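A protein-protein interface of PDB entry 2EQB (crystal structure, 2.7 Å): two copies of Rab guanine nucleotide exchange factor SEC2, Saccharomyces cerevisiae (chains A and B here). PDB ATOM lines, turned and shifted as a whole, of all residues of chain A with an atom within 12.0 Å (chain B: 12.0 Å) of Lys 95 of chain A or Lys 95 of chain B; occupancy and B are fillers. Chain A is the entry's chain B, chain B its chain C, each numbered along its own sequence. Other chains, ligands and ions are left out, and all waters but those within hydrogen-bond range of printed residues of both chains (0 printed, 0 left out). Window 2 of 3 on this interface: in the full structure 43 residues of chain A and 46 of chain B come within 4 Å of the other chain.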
ATOM      1  N   LYS A  86      -6.001  -3.671 -10.997  1.00  0.00           N
ATOM      2  CA  LYS A  86      -4.653  -3.428 -11.504  1.00  0.00           C
ATOM      3  C   LYS A  86      -4.619  -2.226 -12.463  1.00  0.00           C
ATOM      4  O   LYS A  86      -3.837  -1.299 -12.248  1.00  0.00           O
ATOM      5  CB  LYS A  86      -4.106  -4.689 -12.192  1.00  0.00           C
ATOM      6  CG  LYS A  86      -3.892  -5.895 -11.266  1.00  0.00           C
ATOM      7  CD  LYS A  86      -3.432  -7.115 -12.073  1.00  0.00           C
ATOM      8  CE  LYS A  86      -3.379  -8.392 -11.239  1.00  0.00           C
ATOM      9  NZ  LYS A  86      -3.279  -9.590 -12.121  1.00  0.00           N
ATOM     10  N   ARG A  87      -5.456  -2.230 -13.505  1.00  0.00           N
ATOM     11  CA  ARG A  87      -5.495  -1.101 -14.446  1.00  0.00           C
ATOM     12  C   ARG A  87      -5.823   0.265 -13.812  1.00  0.00           C
ATOM     13  O   ARG A  87      -5.250   1.278 -14.212  1.00  0.00           O
ATOM     14  CB  ARG A  87      -6.491  -1.353 -15.582  1.00  0.00           C
ATOM     15  CG  ARG A  87      -6.883  -0.063 -16.307  1.00  0.00           C
ATOM     16  CD  ARG A  87      -7.492  -0.280 -17.693  1.00  0.00           C
ATOM     17  NE  ARG A  87      -6.687  -1.127 -18.579  1.00  0.00           N
ATOM     18  CZ  ARG A  87      -5.354  -1.165 -18.619  1.00  0.00           C
ATOM     19  NH1 ARG A  87      -4.618  -0.409 -17.811  1.00  0.00           N
ATOM     20  NH2 ARG A  87      -4.750  -1.955 -19.494  1.00  0.00           N
ATOM     21  N   LEU A  88      -6.759   0.312 -12.867  1.00  0.00           N
ATOM     22  CA  LEU A  88      -7.077   1.584 -12.204  1.00  0.00           C
ATOM     23  C   LEU A  88      -5.844   1.971 -11.400  1.00  0.00           C
ATOM     24  O   LEU A  88      -5.505   3.144 -11.297  1.00  0.00           O
ATOM     25  CB  LEU A  88      -8.262   1.453 -11.227  1.00  0.00           C
ATOM     26  CG  LEU A  88      -9.707   1.819 -11.595  1.00  0.00           C
ATOM     27  CD1 LEU A  88      -9.917   1.941 -13.103  1.00  0.00           C
ATOM     28  CD2 LEU A  88     -10.610   0.748 -10.999  1.00  0.00           C
ATOM     29  N   THR A  89      -5.173   0.976 -10.826  1.00  0.00           N
ATOM     30  CA  THR A  89      -3.991   1.259 -10.040  1.00  0.00           C
ATOM     31  C   THR A  89      -2.864   1.731 -10.956  1.00  0.00           C
ATOM     32  O   THR A  89      -1.848   2.236 -10.487  1.00  0.00           O
ATOM     33  CB  THR A  89      -3.523   0.025  -9.247  1.00  0.00           C
ATOM     34  OG1 THR A  89      -4.642  -0.587  -8.594  1.00  0.00           O
ATOM     35  CG2 THR A  89      -2.525   0.444  -8.185  1.00  0.00           C
ATOM     36  N   GLU A  90      -3.058   1.574 -12.264  1.00  0.00           N
ATOM     37  CA  GLU A  90      -2.061   1.994 -13.250  1.00  0.00           C
ATOM     38  C   GLU A  90      -2.431   3.348 -13.849  1.00  0.00           C
ATOM     39  O   GLU A  90      -1.585   4.055 -14.398  1.00  0.00           O
ATOM     40  CB  GLU A  90      -1.944   0.959 -14.371  1.00  0.00           C
ATOM     41  CG  GLU A  90      -0.846   1.257 -15.387  1.00  0.00           C
ATOM     42  CD  GLU A  90       0.498   1.519 -14.729  1.00  0.00           C
ATOM     43  OE1 GLU A  90       0.769   0.913 -13.668  1.00  0.00           O
ATOM     44  OE2 GLU A  90       1.288   2.323 -15.279  1.00  0.00           O
ATOM     45  N   GLN A  91      -3.707   3.694 -13.755  1.00  0.00           N
ATOM     46  CA  GLN A  91      -4.186   4.962 -14.276  1.00  0.00           C
ATOM     47  C   GLN A  91      -3.777   6.043 -13.282  1.00  0.00           C
ATOM     48  O   GLN A  91      -3.148   7.040 -13.644  1.00  0.00           O
ATOM     49  CB  GLN A  91      -5.708   4.903 -14.451  1.00  0.00           C
ATOM     50  CG  GLN A  91      -6.128   3.865 -15.489  1.00  0.00           C
ATOM     51  CD  GLN A  91      -7.584   3.963 -15.897  1.00  0.00           C
ATOM     52  OE1 GLN A  91      -7.997   3.368 -16.895  1.00  0.00           O
ATOM     53  NE2 GLN A  91      -8.372   4.710 -15.130  1.00  0.00           N
ATOM     54  N   LEU A  92      -4.130   5.816 -12.022  1.00  0.00           N
ATOM     55  CA  LEU A  92      -3.791   6.715 -10.927  1.00  0.00           C
ATOM     56  C   LEU A  92      -2.317   6.514 -10.601  1.00  0.00           C
ATOM     57  O   LEU A  92      -1.769   7.128  -9.684  1.00  0.00           O
ATOM     58  CB  LEU A  92      -4.650   6.397  -9.702  1.00  0.00           C
ATOM     59  CG  LEU A  92      -4.194   6.835  -8.310  1.00  0.00           C
ATOM     60  CD1 LEU A  92      -5.416   7.100  -7.451  1.00  0.00           C
ATOM     61  CD2 LEU A  92      -3.299   5.756  -7.691  1.00  0.00           C
ATOM     62  N   ARG A  93      -1.677   5.628 -11.351  1.00  0.00           N
ATOM     63  CA  ARG A  93      -0.262   5.386 -11.150  1.00  0.00           C
ATOM     64  C   ARG A  93       0.421   6.549 -11.858  1.00  0.00           C
ATOM     65  O   ARG A  93       1.372   7.134 -11.341  1.00  0.00           O
ATOM     66  CB  ARG A  93       0.136   4.048 -11.776  1.00  0.00           C
ATOM     67  CG  ARG A  93       1.533   3.580 -11.420  1.00  0.00           C
ATOM     68  CD  ARG A  93       2.544   4.008 -12.463  1.00  0.00           C
ATOM     69  NE  ARG A  93       3.906   3.721 -12.030  1.00  0.00           N
ATOM     70  CZ  ARG A  93       4.980   3.855 -12.801  1.00  0.00           C
ATOM     71  NH1 ARG A  93       4.848   4.270 -14.055  1.00  0.00           N
ATOM     72  NH2 ARG A  93       6.184   3.582 -12.316  1.00  0.00           N
ATOM     73  N   GLU A  94      -0.104   6.894 -13.032  1.00  0.00           N
ATOM     74  CA  GLU A  94       0.420   7.994 -13.835  1.00  0.00           C
ATOM     75  C   GLU A  94      -0.025   9.343 -13.279  1.00  0.00           C
ATOM     76  O   GLU A  94       0.815  10.176 -12.943  1.00  0.00           O
ATOM     77  CB  GLU A  94      -0.046   7.850 -15.284  1.00  0.00           C
ATOM     78  CG  GLU A  94       0.483   6.595 -15.959  1.00  0.00           C
ATOM     79  CD  GLU A  94      -0.158   6.339 -17.307  1.00  0.00           C
ATOM     80  OE1 GLU A  94      -0.111   7.241 -18.171  1.00  0.00           O
ATOM     81  OE2 GLU A  94      -0.706   5.232 -17.501  1.00  0.00           O
ATOM     82  N   LYS A  95      -1.339   9.553 -13.190  1.00  0.00           N
ATOM     83  CA  LYS A  95      -1.898  10.800 -12.658  1.00  0.00           C
ATOM     84  C   LYS A  95      -1.057  11.352 -11.508  1.00  0.00           C
ATOM     85  O   LYS A  95      -0.631  12.508 -11.539  1.00  0.00           O
ATOM     86  CB  LYS A  95      -3.332  10.575 -12.166  1.00  0.00           C
ATOM     87  CG  LYS A  95      -4.414  10.716 -13.232  1.00  0.00           C
ATOM     88  CD  LYS A  95      -4.704  12.179 -13.539  1.00  0.00           C
ATOM     89  CE  LYS A  95      -5.987  12.333 -14.347  1.00  0.00           C
ATOM     90  NZ  LYS A  95      -6.320  13.763 -14.599  1.00  0.00           N
ATOM     91  N   ASP A  96      -0.832  10.520 -10.493  1.00  0.00           N
ATOM     92  CA  ASP A  96      -0.032  10.901  -9.332  1.00  0.00           C
ATOM     93  C   ASP A  96       1.208  11.657  -9.789  1.00  0.00           C
ATOM     94  O   ASP A  96       1.432  12.805  -9.401  1.00  0.00           O
ATOM     95  CB  ASP A  96       0.378   9.646  -8.551  1.00  0.00           C
ATOM     96  CG  ASP A  96       1.350   9.945  -7.420  1.00  0.00           C
ATOM     97  OD1 ASP A  96       2.499  10.347  -7.704  1.00  0.00           O
ATOM     98  OD2 ASP A  96       0.962   9.774  -6.244  1.00  0.00           O
ATOM     99  N   THR A  97       2.004  11.004 -10.629  1.00  0.00           N
ATOM    100  CA  THR A  97       3.226  11.596 -11.156  1.00  0.00           C
ATOM    101  C   THR A  97       2.895  12.602 -12.256  1.00  0.00           C
ATOM    102  O   THR A  97       3.031  13.820 -12.004  1.00  0.00           O
ATOM    103  CB  THR A  97       4.154  10.501 -11.728  1.00  0.00           C
ATOM    104  OG1 THR A  97       4.365   9.490 -10.732  1.00  0.00           O
ATOM    105  CG2 THR A  97       5.500  11.090 -12.137  1.00  0.00           C
ATOM    106  OXT THR A  97       2.489  12.162 -13.354  1.00  0.00           O
ATOM    107  N   LYS B  86     -13.711   1.179  -6.075  1.00  0.00           N
ATOM    108  CA  LYS B  86     -14.536   2.365  -5.871  1.00  0.00           C
ATOM    109  C   LYS B  86     -13.571   3.487  -5.482  1.00  0.00           C
ATOM    110  O   LYS B  86     -13.473   4.506  -6.170  1.00  0.00           O
ATOM    111  CB  LYS B  86     -15.546   2.142  -4.731  1.00  0.00           C
ATOM    112  CG  LYS B  86     -16.941   1.662  -5.156  1.00  0.00           C
ATOM    113  CD  LYS B  86     -17.703   2.740  -5.934  1.00  0.00           C
ATOM    114  CE  LYS B  86     -19.192   2.418  -6.090  1.00  0.00           C
ATOM    115  NZ  LYS B  86     -19.987   2.615  -4.838  1.00  0.00           N
ATOM    116  N   ARG B  87     -12.843   3.269  -4.387  1.00  0.00           N
ATOM    117  CA  ARG B  87     -11.880   4.237  -3.879  1.00  0.00           C
ATOM    118  C   ARG B  87     -10.991   4.828  -4.975  1.00  0.00           C
ATOM    119  O   ARG B  87     -10.882   6.047  -5.095  1.00  0.00           O
ATOM    120  CB  ARG B  87     -11.006   3.580  -2.816  1.00  0.00           C
ATOM    121  CG  ARG B  87     -10.079   4.536  -2.083  1.00  0.00           C
ATOM    122  CD  ARG B  87     -10.833   5.381  -1.067  1.00  0.00           C
ATOM    123  NE  ARG B  87      -9.921   6.101  -0.177  1.00  0.00           N
ATOM    124  CZ  ARG B  87      -9.340   7.260  -0.469  1.00  0.00           C
ATOM    125  NH1 ARG B  87      -9.580   7.849  -1.635  1.00  0.00           N
ATOM    126  NH2 ARG B  87      -8.510   7.827   0.402  1.00  0.00           N
ATOM    127  N   LEU B  88     -10.356   3.970  -5.770  1.00  0.00           N
ATOM    128  CA  LEU B  88      -9.473   4.437  -6.842  1.00  0.00           C
ATOM    129  C   LEU B  88     -10.215   5.256  -7.884  1.00  0.00           C
ATOM    130  O   LEU B  88      -9.851   6.398  -8.151  1.00  0.00           O
ATOM    131  CB  LEU B  88      -8.801   3.265  -7.563  1.00  0.00           C
ATOM    132  CG  LEU B  88      -8.017   2.235  -6.760  1.00  0.00           C
ATOM    133  CD1 LEU B  88      -7.310   1.334  -7.752  1.00  0.00           C
ATOM    134  CD2 LEU B  88      -7.017   2.912  -5.827  1.00  0.00           C
ATOM    135  N   THR B  89     -11.240   4.658  -8.490  1.00  0.00           N
ATOM    136  CA  THR B  89     -12.018   5.341  -9.518  1.00  0.00           C
ATOM    137  C   THR B  89     -12.289   6.748  -9.045  1.00  0.00           C
ATOM    138  O   THR B  89     -12.237   7.705  -9.821  1.00  0.00           O
ATOM    139  CB  THR B  89     -13.374   4.664  -9.772  1.00  0.00           C
ATOM    140  OG1 THR B  89     -13.174   3.311 -10.204  1.00  0.00           O
ATOM    141  CG2 THR B  89     -14.140   5.426 -10.843  1.00  0.00           C
ATOM    142  N   GLU B  90     -12.574   6.852  -7.752  1.00  0.00           N
ATOM    143  CA  GLU B  90     -12.864   8.127  -7.108  1.00  0.00           C
ATOM    144  C   GLU B  90     -11.611   8.980  -6.886  1.00  0.00           C
ATOM    145  O   GLU B  90     -11.685  10.205  -6.931  1.00  0.00           O
ATOM    146  CB  GLU B  90     -13.597   7.859  -5.794  1.00  0.00           C
ATOM    147  CG  GLU B  90     -13.332   8.828  -4.666  1.00  0.00           C
ATOM    148  CD  GLU B  90     -13.464   8.147  -3.313  1.00  0.00           C
ATOM    149  OE1 GLU B  90     -14.473   7.432  -3.099  1.00  0.00           O
ATOM    150  OE2 GLU B  90     -12.560   8.324  -2.467  1.00  0.00           O
ATOM    151  N   GLN B  91     -10.465   8.344  -6.653  1.00  0.00           N
ATOM    152  CA  GLN B  91      -9.222   9.093  -6.477  1.00  0.00           C
ATOM    153  C   GLN B  91      -8.763   9.541  -7.864  1.00  0.00           C
ATOM    154  O   GLN B  91      -7.789  10.275  -7.997  1.00  0.00           O
ATOM    155  CB  GLN B  91      -8.126   8.225  -5.846  1.00  0.00           C
ATOM    156  CG  GLN B  91      -8.472   7.615  -4.498  1.00  0.00           C
ATOM    157  CD  GLN B  91      -7.486   6.535  -4.095  1.00  0.00           C
ATOM    158  OE1 GLN B  91      -6.315   6.812  -3.844  1.00  0.00           O
ATOM    159  NE2 GLN B  91      -7.955   5.292  -4.045  1.00  0.00           N
ATOM    160  N   LEU B  92      -9.469   9.079  -8.893  1.00  0.00           N
ATOM    161  CA  LEU B  92      -9.149   9.435 -10.272  1.00  0.00           C
ATOM    162  C   LEU B  92      -9.933  10.649 -10.732  1.00  0.00           C
ATOM    163  O   LEU B  92     -10.022  10.934 -11.929  1.00  0.00           O
ATOM    164  CB  LEU B  92      -9.447   8.277 -11.222  1.00  0.00           C
ATOM    165  CG  LEU B  92      -8.449   7.127 -11.294  1.00  0.00           C
ATOM    166  CD1 LEU B  92      -8.560   6.516 -12.674  1.00  0.00           C
ATOM    167  CD2 LEU B  92      -7.037   7.622 -11.075  1.00  0.00           C
ATOM    168  N   ARG B  93     -10.529  11.343  -9.774  1.00  0.00           N
ATOM    169  CA  ARG B  93     -11.280  12.558 -10.051  1.00  0.00           C
ATOM    170  C   ARG B  93     -10.583  13.596  -9.192  1.00  0.00           C
ATOM    171  O   ARG B  93     -10.509  14.771  -9.542  1.00  0.00           O
ATOM    172  CB  ARG B  93     -12.735  12.406  -9.617  1.00  0.00           C
ATOM    173  CG  ARG B  93     -13.480  11.316 -10.348  1.00  0.00           C
ATOM    174  CD  ARG B  93     -14.715  10.927  -9.572  1.00  0.00           C
ATOM    175  NE  ARG B  93     -15.423   9.812 -10.191  1.00  0.00           N
ATOM    176  CZ  ARG B  93     -16.246   9.005  -9.532  1.00  0.00           C
ATOM    177  NH1 ARG B  93     -16.456   9.192  -8.234  1.00  0.00           N
ATOM    178  NH2 ARG B  93     -16.861   8.016 -10.169  1.00  0.00           N
ATOM    179  N   GLU B  94     -10.068  13.122  -8.058  1.00  0.00           N
ATOM    180  CA  GLU B  94      -9.332  13.950  -7.114  1.00  0.00           C
ATOM    181  C   GLU B  94      -7.938  14.171  -7.703  1.00  0.00           C
ATOM    182  O   GLU B  94      -7.028  14.660  -7.031  1.00  0.00           O
ATOM    183  CB  GLU B  94      -9.251  13.250  -5.747  1.00  0.00           C
ATOM    184  CG  GLU B  94     -10.556  13.311  -4.936  1.00  0.00           C
ATOM    185  CD  GLU B  94     -10.648  12.262  -3.828  1.00  0.00           C
ATOM    186  OE1 GLU B  94      -9.658  12.069  -3.089  1.00  0.00           O
ATOM    187  OE2 GLU B  94     -11.722  11.638  -3.687  1.00  0.00           O
ATOM    188  N   LYS B  95      -7.793  13.787  -8.970  1.00  0.00           N
ATOM    189  CA  LYS B  95      -6.552  13.943  -9.723  1.00  0.00           C
ATOM    190  C   LYS B  95      -6.882  14.611 -11.058  1.00  0.00           C
ATOM    191  O   LYS B  95      -5.998  14.889 -11.867  1.00  0.00           O
ATOM    192  CB  LYS B  95      -5.877  12.586  -9.957  1.00  0.00           C
ATOM    193  CG  LYS B  95      -5.191  12.020  -8.717  1.00  0.00           C
ATOM    194  CD  LYS B  95      -4.140  12.988  -8.181  1.00  0.00           C
ATOM    195  CE  LYS B  95      -3.455  12.452  -6.929  1.00  0.00           C
ATOM    196  NZ  LYS B  95      -2.643  11.228  -7.191  1.00  0.00           N
ATOM    197  N   ASP B  96      -8.172  14.848 -11.275  1.00  0.00           N
ATOM    198  CA  ASP B  96      -8.661  15.518 -12.473  1.00  0.00           C
ATOM    199  C   ASP B  96      -9.268  16.821 -11.982  1.00  0.00           C
ATOM    200  O   ASP B  96      -9.481  17.762 -12.749  1.00  0.00           O
ATOM    201  CB  ASP B  96      -9.734  14.681 -13.175  1.00  0.00           C
ATOM    202  CG  ASP B  96     -10.438  15.448 -14.280  1.00  0.00           C
ATOM    203  OD1 ASP B  96     -11.235  16.356 -13.960  1.00  0.00           O
ATOM    204  OD2 ASP B  96     -10.187  15.151 -15.468  1.00  0.00           O
ATOM    205  N   THR B  97      -9.539  16.855 -10.681  1.00  0.00           N
ATOM    206  CA  THR B  97     -10.109  18.025 -10.033  1.00  0.00           C
ATOM    207  C   THR B  97      -8.953  18.884  -9.502  1.00  0.00           C
ATOM    208  O   THR B  97      -8.975  19.289  -8.319  1.00  0.00           O
ATOM    209  CB  THR B  97     -11.056  17.600  -8.873  1.00  0.00           C
ATOM    210  OG1 THR B  97     -11.860  18.715  -8.474  1.00  0.00           O
ATOM    211  CG2 THR B  97     -10.261  17.088  -7.670  1.00  0.00           C
ATOM    212  OXT THR B  97      -8.025  19.150 -10.297  1.00  0.00           O
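Of the 12 printed residues of chain B, 6 touch a printed residue of chain A. Hydrophobic or aromatic side chains of chain B that line the printed part of chain A: Leu 88 and Leu 92. Hydrophobic or aromatic side chains of chain A within 4 Å of the printed part of chain B: Leu 88 and Leu 92.
The backbone NH (N) of Leu 88 of chain B lies close to the side-chain amide nitrogen (NE2) of Gln 91 of chain B, 3.2 Å away. The backbone carbonyl oxygen (O) of Arg 87 of chain B sits close to the side-chain amide nitrogen (NE2) of Gln 91 of chain B (3.2 Å).
Leu 88 of chain B touches Leu 88 of chain A (CD1 to CB, 3.6 Å). Thr 89 of chain B touches Leu 88 of chain A. Thr 89 of chain A touches Leu 88 of chain B (OG1 to CD1, 3.4 Å). CD1 of Leu 92 of chain B touches NE2 of Gln 91 of chain A (3.1 Å). CB of Gln 91 of chain B touches CD1 of Leu 92 of chain A (3.3 Å). Leu 92 of chain A touches Leu 92 of chain B. Lys 95 of chain A touches Asp 96 of chain B (NZ to CA, 3.6 Å). Asp 96 of chain A touches Lys 95 of chain B (CA to NZ, 3.4 Å).
Of chain B, only Lys 95 and Asp 96 come within 4 Å of Lys 95 of chain A. Printed residues of chain A within 4 Å of Lys 95 of chain B: Lys 95 and Asp 96. No residue of chain B comes within 4 Å of Glu 94 of chain A. No residue of chain B comes within 4 Å of Thr 97 of chain A. Of chain A, only Gln 91 (3.1 Å) and Leu 92 (3.0 Å) come within 4 Å of Leu 92 of chain B. Glu 94 of chain B touches none of the printed residues of chain A. Asp 96 of chain B touches just one residue of chain A: Lys 95 (3.6 Å). Printed residues of chain A within 4 Å of Leu 88 of chain B: Leu 88 (3.6 Å) and Thr 89 (3.4 Å). Of the printed residues of chain B, Thr 89 of chain A touches Leu 88. Printed residues of chain B within 4 Å of Gln 91 of chain A: Leu 92 (3.1 Å). Arg 93 of chain B touches none of the printed residues of chain A. The nearest residue of chain A that does not touch Lys 95 of chain B is Leu 92 of chain A (4.8 Å). The nearest printed residue of chain A that does not touch Thr 89 of chain B is Leu 92 of chain A (6.4 Å).
Leu 88 of chain B touches its own counterpart, Leu 88 of chain A. Leu 88 of chain A touches Thr 89 of chain B, and with the chains exchanged Thr 89 of chain A touches Leu 88 of chain B. Lys 95 of chain B touches its own counterpart, Lys 95 of chain A. Lys 95 of chain A touches Asp 96 of chain B, and with the chains exchanged Asp 96 of chain A touches Lys 95 of chain B. 12 positions are printed for both chains. Of the 9 pairs that touch across the chains among the printed residues, 9 have their exchanged pair printed and touching as well.
NZ of Lys 95 of chain A is in hydrogen-bond range of O of Lys 95 of chain B (3.0 Å).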
